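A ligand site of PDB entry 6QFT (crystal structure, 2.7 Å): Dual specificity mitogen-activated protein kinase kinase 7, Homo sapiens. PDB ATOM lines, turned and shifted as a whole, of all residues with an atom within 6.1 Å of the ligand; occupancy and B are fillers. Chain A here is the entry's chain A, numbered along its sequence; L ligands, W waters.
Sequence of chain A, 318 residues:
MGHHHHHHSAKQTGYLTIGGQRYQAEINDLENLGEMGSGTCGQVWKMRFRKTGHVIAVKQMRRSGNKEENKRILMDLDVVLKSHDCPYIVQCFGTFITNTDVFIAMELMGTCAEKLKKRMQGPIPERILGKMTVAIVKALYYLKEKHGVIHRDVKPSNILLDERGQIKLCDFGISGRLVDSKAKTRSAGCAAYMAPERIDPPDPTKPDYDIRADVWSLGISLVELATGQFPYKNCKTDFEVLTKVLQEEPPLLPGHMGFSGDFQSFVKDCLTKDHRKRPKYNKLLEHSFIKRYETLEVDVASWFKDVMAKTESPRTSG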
ATOM      1  N   MET A  36      -3.538  -0.901  -2.066  1.00  0.00           N
ATOM      2  CA  MET A  36      -2.261  -0.332  -1.640  1.00  0.00           C
ATOM      3  C   MET A  36      -1.161  -1.360  -1.873  1.00  0.00           C
ATOM      4  O   MET A  36      -1.288  -2.518  -1.468  1.00  0.00           O
ATOM      5  CB  MET A  36      -2.307   0.068  -0.165  1.00  0.00           C
ATOM      6  CG  MET A  36      -3.614   0.691   0.269  1.00  0.00           C
ATOM      7  SD  MET A  36      -3.525   1.319   1.960  1.00  0.00           S
ATOM      8  CE  MET A  36      -2.242   2.554   1.767  1.00  0.00           C
ATOM      9  N   GLY A  37      -0.076  -0.920  -2.514  1.00  0.00           N
ATOM     10  CA  GLY A  37       1.047  -1.815  -2.745  1.00  0.00           C
ATOM     11  C   GLY A  37       0.671  -2.973  -3.659  1.00  0.00           C
ATOM     12  O   GLY A  37      -0.209  -2.865  -4.523  1.00  0.00           O
ATOM     13  N   SER A  38       1.352  -4.093  -3.457  1.00  0.00           N
ATOM     14  CA  SER A  38       1.125  -5.282  -4.266  1.00  0.00           C
ATOM     15  C   SER A  38       1.774  -6.491  -3.603  1.00  0.00           C
ATOM     16  O   SER A  38       2.904  -6.397  -3.106  1.00  0.00           O
ATOM     17  CB  SER A  38       1.685  -5.100  -5.688  1.00  0.00           C
ATOM     18  OG  SER A  38       1.591  -6.309  -6.429  1.00  0.00           O
ATOM     19  N   GLY A  39       1.057  -7.606  -3.601  1.00  0.00           N
ATOM     20  CA  GLY A  39       1.640  -8.871  -3.181  1.00  0.00           C
ATOM     21  C   GLY A  39       1.988  -8.907  -1.706  1.00  0.00           C
ATOM     22  O   GLY A  39       1.192  -8.506  -0.839  1.00  0.00           O
ATOM     23  N   THR A  40       3.198  -9.391  -1.416  1.00  0.00           N
ATOM     24  CA  THR A  40       3.719  -9.585  -0.057  1.00  0.00           C
ATOM     25  C   THR A  40       2.774 -10.517   0.692  1.00  0.00           C
ATOM     26  O   THR A  40       2.542 -11.634   0.196  1.00  0.00           O
ATOM     27  CB  THR A  40       3.968  -8.222   0.614  1.00  0.00           C
ATOM     28  OG1 THR A  40       2.719  -7.543   0.812  1.00  0.00           O
ATOM     29  CG2 THR A  40       4.885  -7.361  -0.258  1.00  0.00           C
ATOM     30  N   CYS A  41       2.222 -10.134   1.843  1.00  0.00           N
ATOM     31  CA  CYS A  41       1.398 -11.062   2.623  1.00  0.00           C
ATOM     32  C   CYS A  41       0.084 -11.352   1.907  1.00  0.00           C
ATOM     33  O   CYS A  41      -0.218 -12.507   1.574  1.00  0.00           O
ATOM     34  CB  CYS A  41       1.145 -10.486   4.019  1.00  0.00           C
ATOM     35  SG  CYS A  41       0.347 -11.631   5.168  1.00  0.00           S
ATOM     36  N   GLY A  42      -0.719 -10.327   1.673  1.00  0.00           N
ATOM     37  CA  GLY A  42      -2.009 -10.495   1.013  1.00  0.00           C
ATOM     38  C   GLY A  42      -2.425  -9.210   0.329  1.00  0.00           C
ATOM     39  O   GLY A  42      -1.725  -8.196   0.380  1.00  0.00           O
ATOM     40  N   VAL A  44      -4.110  -5.920   0.059  1.00  0.00           N
ATOM     41  CA  VAL A  44      -4.485  -4.904   1.032  1.00  0.00           C
ATOM     42  C   VAL A  44      -5.208  -3.778   0.299  1.00  0.00           C
ATOM     43  O   VAL A  44      -4.645  -3.144  -0.593  1.00  0.00           O
ATOM     44  CB  VAL A  44      -3.257  -4.360   1.789  1.00  0.00           C
ATOM     45  CG1 VAL A  44      -3.701  -3.349   2.836  1.00  0.00           C
ATOM     46  CG2 VAL A  44      -2.491  -5.500   2.442  1.00  0.00           C
ATOM     47  N   ALA A  57      -6.856   0.354   6.420  1.00  0.00           N
ATOM     48  CA  ALA A  57      -6.339  -0.662   5.520  1.00  0.00           C
ATOM     49  C   ALA A  57      -7.042  -1.982   5.805  1.00  0.00           C
ATOM     50  O   ALA A  57      -7.282  -2.334   6.960  1.00  0.00           O
ATOM     51  CB  ALA A  57      -4.824  -0.824   5.677  1.00  0.00           C
ATOM     52  N   LYS A  59      -7.059  -6.101   4.743  1.00  0.00           N
ATOM     53  CA  LYS A  59      -6.537  -7.300   4.107  1.00  0.00           C
ATOM     54  C   LYS A  59      -7.686  -8.214   3.711  1.00  0.00           C
ATOM     55  O   LYS A  59      -8.610  -8.432   4.501  1.00  0.00           O
ATOM     56  CB  LYS A  59      -5.586  -8.055   5.038  1.00  0.00           C
ATOM     57  CG  LYS A  59      -4.108  -7.786   4.825  1.00  0.00           C
ATOM     58  CD  LYS A  59      -3.278  -8.693   5.716  1.00  0.00           C
ATOM     59  CE  LYS A  59      -1.793  -8.501   5.471  1.00  0.00           C
ATOM     60  NZ  LYS A  59      -0.964  -9.365   6.347  1.00  0.00           N
ATOM     61  N   ASP A  76       0.099 -14.250  10.541  1.00  0.00           N
ATOM     62  CA  ASP A  76       0.300 -12.829  10.789  1.00  0.00           C
ATOM     63  C   ASP A  76      -0.804 -12.263  11.679  1.00  0.00           C
ATOM     64  O   ASP A  76      -0.527 -11.576  12.663  1.00  0.00           O
ATOM     65  CB  ASP A  76       0.368 -12.072   9.452  1.00  0.00           C
ATOM     66  CG  ASP A  76       0.475 -10.562   9.637  1.00  0.00           C
ATOM     67  OD1 ASP A  76       1.576 -10.081   9.964  1.00  0.00           O
ATOM     68  OD2 ASP A  76      -0.544  -9.870   9.456  1.00  0.00           O
ATOM     69  N   VAL A  90       1.664  -2.815  14.073  1.00  0.00           N
ATOM     70  CA  VAL A  90       0.416  -2.336  13.498  1.00  0.00           C
ATOM     71  C   VAL A  90      -0.761  -3.053  14.148  1.00  0.00           C
ATOM     72  O   VAL A  90      -0.769  -4.286  14.266  1.00  0.00           O
ATOM     73  CB  VAL A  90       0.426  -2.497  11.978  1.00  0.00           C
ATOM     74  CG1 VAL A  90       1.403  -1.523  11.344  1.00  0.00           C
ATOM     75  CG2 VAL A  90       0.771  -3.927  11.589  1.00  0.00           C
ATOM     76  N   GLN A  91      -1.754  -2.284  14.573  1.00  0.00           N
ATOM     77  CA  GLN A  91      -2.903  -2.829  15.293  1.00  0.00           C
ATOM     78  C   GLN A  91      -3.986  -3.283  14.330  1.00  0.00           C
ATOM     79  O   GLN A  91      -4.172  -2.709  13.254  1.00  0.00           O
ATOM     80  CB  GLN A  91      -3.474  -1.797  16.264  1.00  0.00           C
ATOM     81  CG  GLN A  91      -3.137  -2.045  17.721  1.00  0.00           C
ATOM     82  CD  GLN A  91      -1.645  -2.075  17.984  1.00  0.00           C
ATOM     83  OE1 GLN A  91      -1.059  -3.146  18.199  1.00  0.00           O
ATOM     84  NE2 GLN A  91      -1.017  -0.910  17.988  1.00  0.00           N
ATOM     85  N   MET A 106      -6.870  -3.359   9.320  1.00  0.00           N
ATOM     86  CA  MET A 106      -5.618  -2.909   9.919  1.00  0.00           C
ATOM     87  C   MET A 106      -5.582  -1.385   9.921  1.00  0.00           C
ATOM     88  O   MET A 106      -6.233  -0.730   9.100  1.00  0.00           O
ATOM     89  CB  MET A 106      -4.405  -3.461   9.168  1.00  0.00           C
ATOM     90  CG  MET A 106      -4.259  -4.974   9.234  1.00  0.00           C
ATOM     91  SD  MET A 106      -3.813  -5.564  10.872  1.00  0.00           S
ATOM     92  CE  MET A 106      -3.388  -7.272  10.525  1.00  0.00           C
ATOM     93  N   GLU A 107      -4.802  -0.821  10.847  1.00  0.00           N
ATOM     94  CA  GLU A 107      -4.640   0.620  10.885  1.00  0.00           C
ATOM     95  C   GLU A 107      -3.881   1.098   9.653  1.00  0.00           C
ATOM     96  O   GLU A 107      -2.994   0.398   9.143  1.00  0.00           O
ATOM     97  CB  GLU A 107      -3.896   1.045  12.155  1.00  0.00           C
ATOM     98  CG  GLU A 107      -2.434   0.651  12.209  1.00  0.00           C
ATOM     99  CD  GLU A 107      -1.726   1.172  13.436  1.00  0.00           C
ATOM    100  OE1 GLU A 107      -1.469   0.372  14.368  1.00  0.00           O
ATOM    101  OE2 GLU A 107      -1.432   2.389  13.481  1.00  0.00           O
ATOM    102  N   LEU A 108      -4.235   2.277   9.161  1.00  0.00           N
ATOM    103  CA  LEU A 108      -3.652   2.803   7.942  1.00  0.00           C
ATOM    104  C   LEU A 108      -2.314   3.473   8.236  1.00  0.00           C
ATOM    105  O   LEU A 108      -2.262   4.451   8.986  1.00  0.00           O
ATOM    106  CB  LEU A 108      -4.603   3.782   7.261  1.00  0.00           C
ATOM    107  CG  LEU A 108      -4.085   4.388   5.951  1.00  0.00           C
ATOM    108  CD1 LEU A 108      -3.796   3.288   4.950  1.00  0.00           C
ATOM    109  CD2 LEU A 108      -5.075   5.393   5.391  1.00  0.00           C
ATOM    110  N   MET A 109      -1.242   2.938   7.666  1.00  0.00           N
ATOM    111  CA  MET A 109       0.063   3.556   7.731  1.00  0.00           C
ATOM    112  C   MET A 109       0.381   4.243   6.401  1.00  0.00           C
ATOM    113  O   MET A 109      -0.248   3.969   5.373  1.00  0.00           O
ATOM    114  CB  MET A 109       1.146   2.526   8.058  1.00  0.00           C
ATOM    115  CG  MET A 109       0.916   1.769   9.369  1.00  0.00           C
ATOM    116  SD  MET A 109       1.063   2.822  10.831  1.00  0.00           S
ATOM    117  CE  MET A 109       2.811   3.239  10.791  1.00  0.00           C
ATOM    118  N   GLY A 110       1.346   5.152   6.447  1.00  0.00           N
ATOM    119  CA  GLY A 110       1.730   5.885   5.246  1.00  0.00           C
ATOM    120  C   GLY A 110       2.385   4.992   4.211  1.00  0.00           C
ATOM    121  O   GLY A 110       1.812   4.736   3.150  1.00  0.00           O
ATOM    122  N   THR A 111       3.590   4.522   4.510  1.00  0.00           N
ATOM    123  CA  THR A 111       4.336   3.680   3.585  1.00  0.00           C
ATOM    124  C   THR A 111       5.458   2.983   4.345  1.00  0.00           C
ATOM    125  O   THR A 111       5.664   3.226   5.537  1.00  0.00           O
ATOM    126  CB  THR A 111       4.900   4.511   2.423  1.00  0.00           C
ATOM    127  OG1 THR A 111       5.421   3.627   1.422  1.00  0.00           O
ATOM    128  CG2 THR A 111       6.005   5.432   2.910  1.00  0.00           C
ATOM    129  N   CYS A 112       6.167   2.114   3.634  1.00  0.00           N
ATOM    130  CA  CYS A 112       7.283   1.389   4.224  1.00  0.00           C
ATOM    131  C   CYS A 112       8.580   2.175   4.050  1.00  0.00           C
ATOM    132  O   CYS A 112       8.658   3.140   3.291  1.00  0.00           O
ATOM    133  CB  CYS A 112       7.406  -0.006   3.607  1.00  0.00           C
ATOM    134  SG  CYS A 112       7.690  -0.021   1.830  1.00  0.00           S
ATOM    135  N   ALA A 113       9.609   1.742   4.783  1.00  0.00           N
ATOM    136  CA  ALA A 113      10.902   2.410   4.710  1.00  0.00           C
ATOM    137  C   ALA A 113      11.553   2.249   3.341  1.00  0.00           C
ATOM    138  O   ALA A 113      12.335   3.107   2.924  1.00  0.00           O
ATOM    139  CB  ALA A 113      11.834   1.883   5.801  1.00  0.00           C
ATOM    140  N   GLU A 114      11.241   1.154   2.641  1.00  0.00           N
ATOM    141  CA  GLU A 114      11.783   0.965   1.301  1.00  0.00           C
ATOM    142  C   GLU A 114      11.289   2.041   0.343  1.00  0.00           C
ATOM    143  O   GLU A 114      12.072   2.609  -0.425  1.00  0.00           O
ATOM    144  CB  GLU A 114      11.414  -0.424   0.779  1.00  0.00           C
ATOM    145  CG  GLU A 114      11.697  -0.622  -0.702  1.00  0.00           C
ATOM    146  CD  GLU A 114      11.237  -1.969  -1.208  1.00  0.00           C
ATOM    147  OE1 GLU A 114      12.093  -2.833  -1.497  1.00  0.00           O
ATOM    148  OE2 GLU A 114      10.008  -2.180  -1.310  1.00  0.00           O
ATOM    149  N   LYS A 115       9.988   2.326   0.379  1.00  0.00           N
ATOM    150  CA  LYS A 115       9.441   3.380  -0.481  1.00  0.00           C
ATOM    151  C   LYS A 115       9.906   4.765  -0.036  1.00  0.00           C
ATOM    152  O   LYS A 115      10.053   5.664  -0.879  1.00  0.00           O
ATOM    153  CB  LYS A 115       7.910   3.310  -0.492  1.00  0.00           C
ATOM    154  N   PRO A 156      13.492  -3.238   5.305  1.00  0.00           N
ATOM    155  CA  PRO A 156      12.847  -1.911   5.179  1.00  0.00           C
ATOM    156  C   PRO A 156      11.411  -1.981   4.682  1.00  0.00           C
ATOM    157  O   PRO A 156      10.622  -1.080   4.985  1.00  0.00           O
ATOM    158  CB  PRO A 156      13.753  -1.185   4.187  1.00  0.00           C
ATOM    159  CG  PRO A 156      15.079  -1.822   4.342  1.00  0.00           C
ATOM    160  CD  PRO A 156      14.806  -3.276   4.637  1.00  0.00           C
ATOM    161  N   SER A 157      11.048  -3.020   3.929  1.00  0.00           N
ATOM    162  CA  SER A 157       9.668  -3.161   3.477  1.00  0.00           C
ATOM    163  C   SER A 157       8.721  -3.513   4.609  1.00  0.00           C
ATOM    164  O   SER A 157       7.503  -3.318   4.470  1.00  0.00           O
ATOM    165  CB  SER A 157       9.578  -4.212   2.366  1.00  0.00           C
ATOM    166  OG  SER A 157       9.996  -5.480   2.834  1.00  0.00           O
ATOM    167  N   ASN A 158       9.236  -4.022   5.726  1.00  0.00           N
ATOM    168  CA  ASN A 158       8.415  -4.370   6.882  1.00  0.00           C
ATOM    169  C   ASN A 158       8.390  -3.279   7.939  1.00  0.00           C
ATOM    170  O   ASN A 158       7.800  -3.486   9.006  1.00  0.00           O
ATOM    171  CB  ASN A 158       8.913  -5.687   7.504  1.00  0.00           C
ATOM    172  CG  ASN A 158       8.715  -6.873   6.590  1.00  0.00           C
ATOM    173  OD1 ASN A 158       7.714  -6.954   5.863  1.00  0.00           O
ATOM    174  ND2 ASN A 158       9.653  -7.807   6.609  1.00  0.00           N
ATOM    175  N   LEU A 160       6.948   0.231   8.673  1.00  0.00           N
ATOM    176  CA  LEU A 160       5.953   1.175   8.200  1.00  0.00           C
ATOM    177  C   LEU A 160       6.029   2.476   8.989  1.00  0.00           C
ATOM    178  O   LEU A 160       6.254   2.469  10.201  1.00  0.00           O
ATOM    179  CB  LEU A 160       4.549   0.593   8.299  1.00  0.00           C
ATOM    180  CG  LEU A 160       4.267  -0.722   7.563  1.00  0.00           C
ATOM    181  CD1 LEU A 160       2.783  -1.040   7.594  1.00  0.00           C
ATOM    182  CD2 LEU A 160       4.777  -0.656   6.130  1.00  0.00           C
ATOM    183  N   CYS A 170       5.089  -4.820  10.609  1.00  0.00           N
ATOM    184  CA  CYS A 170       3.801  -5.153  10.004  1.00  0.00           C
ATOM    185  C   CYS A 170       3.622  -6.637   9.685  1.00  0.00           C
ATOM    186  O   CYS A 170       2.583  -7.222   9.996  1.00  0.00           O
ATOM    187  CB  CYS A 170       3.575  -4.327   8.739  1.00  0.00           C
ATOM    188  SG  CYS A 170       4.735  -4.642   7.392  1.00  0.00           S
HETATM  189  C1  LIG L   1       6.350  -1.091   1.617  1.00  0.00           C
HETATM  190  C2  LIG L   1       0.098  -1.368   4.569  1.00  0.00           C
HETATM  191  C3  LIG L   1       1.320  -2.586   2.625  1.00  0.00           C
HETATM  192  N1  LIG L   1      -1.651  -1.280   7.928  1.00  0.00           N
HETATM  193  C4  LIG L   1      -1.111  -0.902   6.754  1.00  0.00           C
HETATM  194  C5  LIG L   1       4.286  -2.354   1.091  1.00  0.00           C
HETATM  195  N2  LIG L   1       0.619  -2.439   3.930  1.00  0.00           N
HETATM  196  C6  LIG L   1       0.587  -3.604   1.770  1.00  0.00           C
HETATM  197  C7  LIG L   1       5.000  -1.519   2.138  1.00  0.00           C
HETATM  198  N3  LIG L   1      -1.135   0.396   6.355  1.00  0.00           N
HETATM  199  C8  LIG L   1      -0.601   0.783   5.177  1.00  0.00           C
HETATM  200  O1  LIG L   1       4.599  -2.263  -0.079  1.00  0.00           O
HETATM  201  C9  LIG L   1      -0.468  -1.870   5.839  1.00  0.00           C
HETATM  202  C10 LIG L   1      -0.170  -3.318   5.770  1.00  0.00           C
HETATM  203  C11 LIG L   1       1.324  -3.817   0.444  1.00  0.00           C
HETATM  204  C12 LIG L   1       2.776  -4.212   0.682  1.00  0.00           C
HETATM  205  C13 LIG L   1       2.748  -3.063   2.858  1.00  0.00           C
HETATM  206  I1  LIG L   1      -0.707  -4.720   7.296  1.00  0.00           I
HETATM  207  N4  LIG L   1      -0.001  -0.049   4.301  1.00  0.00           N
HETATM  208  N5  LIG L   1       0.471  -3.659   4.638  1.00  0.00           N
HETATM  209  N6  LIG L   1       3.321  -3.163   1.528  1.00  0.00           N
HETATM  210  O   HOH W   1       1.616  -6.650   4.730  1.00  0.00           O
HETATM  211  O   HOH W   2       0.116  -7.473   8.992  1.00  0.00           O
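O of Glu 107 is in hydrogen-bond range of N1 of the ligand (2.5 Å).
N of Met 109 lies within hydrogen-bond range of N3 of the ligand (2.9 Å).
SG of Cys 112 is covalently linked to C1 of the ligand, 1.7 Å away.
Water W2 lies within hydrogen-bond range of the side-chain carboxylate of Asp 76 (2.5 Å), the backbone carbonyl oxygen of Cys 170 (2.7 Å) and the side-chain amino group of Lys 59 (3.4 Å).
Met 36 touches the ligand.
Gly 37 touches the ligand.
Ser 38 touches the ligand (N to C11, 3.9 Å).
Thr 40 touches the ligand (OG1 to C12, 3.3 Å).
Val 44 touches the ligand (CG2 to C6, 3.7 Å).
Ala 57 touches the ligand.
CB of Met 106 touches N1 of the ligand, at 3.7 Å.
Leu 108 touches the ligand.
Ser 157 touches the ligand (O to C1, 3.8 Å).
Leu 160 touches the ligand (CD1 to C9, 3.8 Å).
Within 4 Å of the ligand: Met 36, Gly 37, Ser 38, Thr 40, Val 44, Ala 57, Met 106, Glu 107, Leu 108, Met 109, Cys 112, Ser 157 and Leu 160.
The nearest printed residue that does not touch the ligand is Lys 59 (4.3 Å).
The backbone NH of Gln 91 sits at hydrogen-bond distance from the side-chain carboxylate of Glu 107 (2.7 Å).
The backbone carbonyl oxygen (O) of Val 44 sits at hydrogen-bond distance from the backbone NH (N) of Met 36 (2.9 Å).
The backbone NH of Met 106 lies within hydrogen-bond range of the backbone carbonyl oxygen of Ala 57 (2.6 Å).
The backbone NH (N) of Lys 115 sits at hydrogen-bond distance from the side-chain sulfur (SG) of Cys 112 (3.6 Å).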
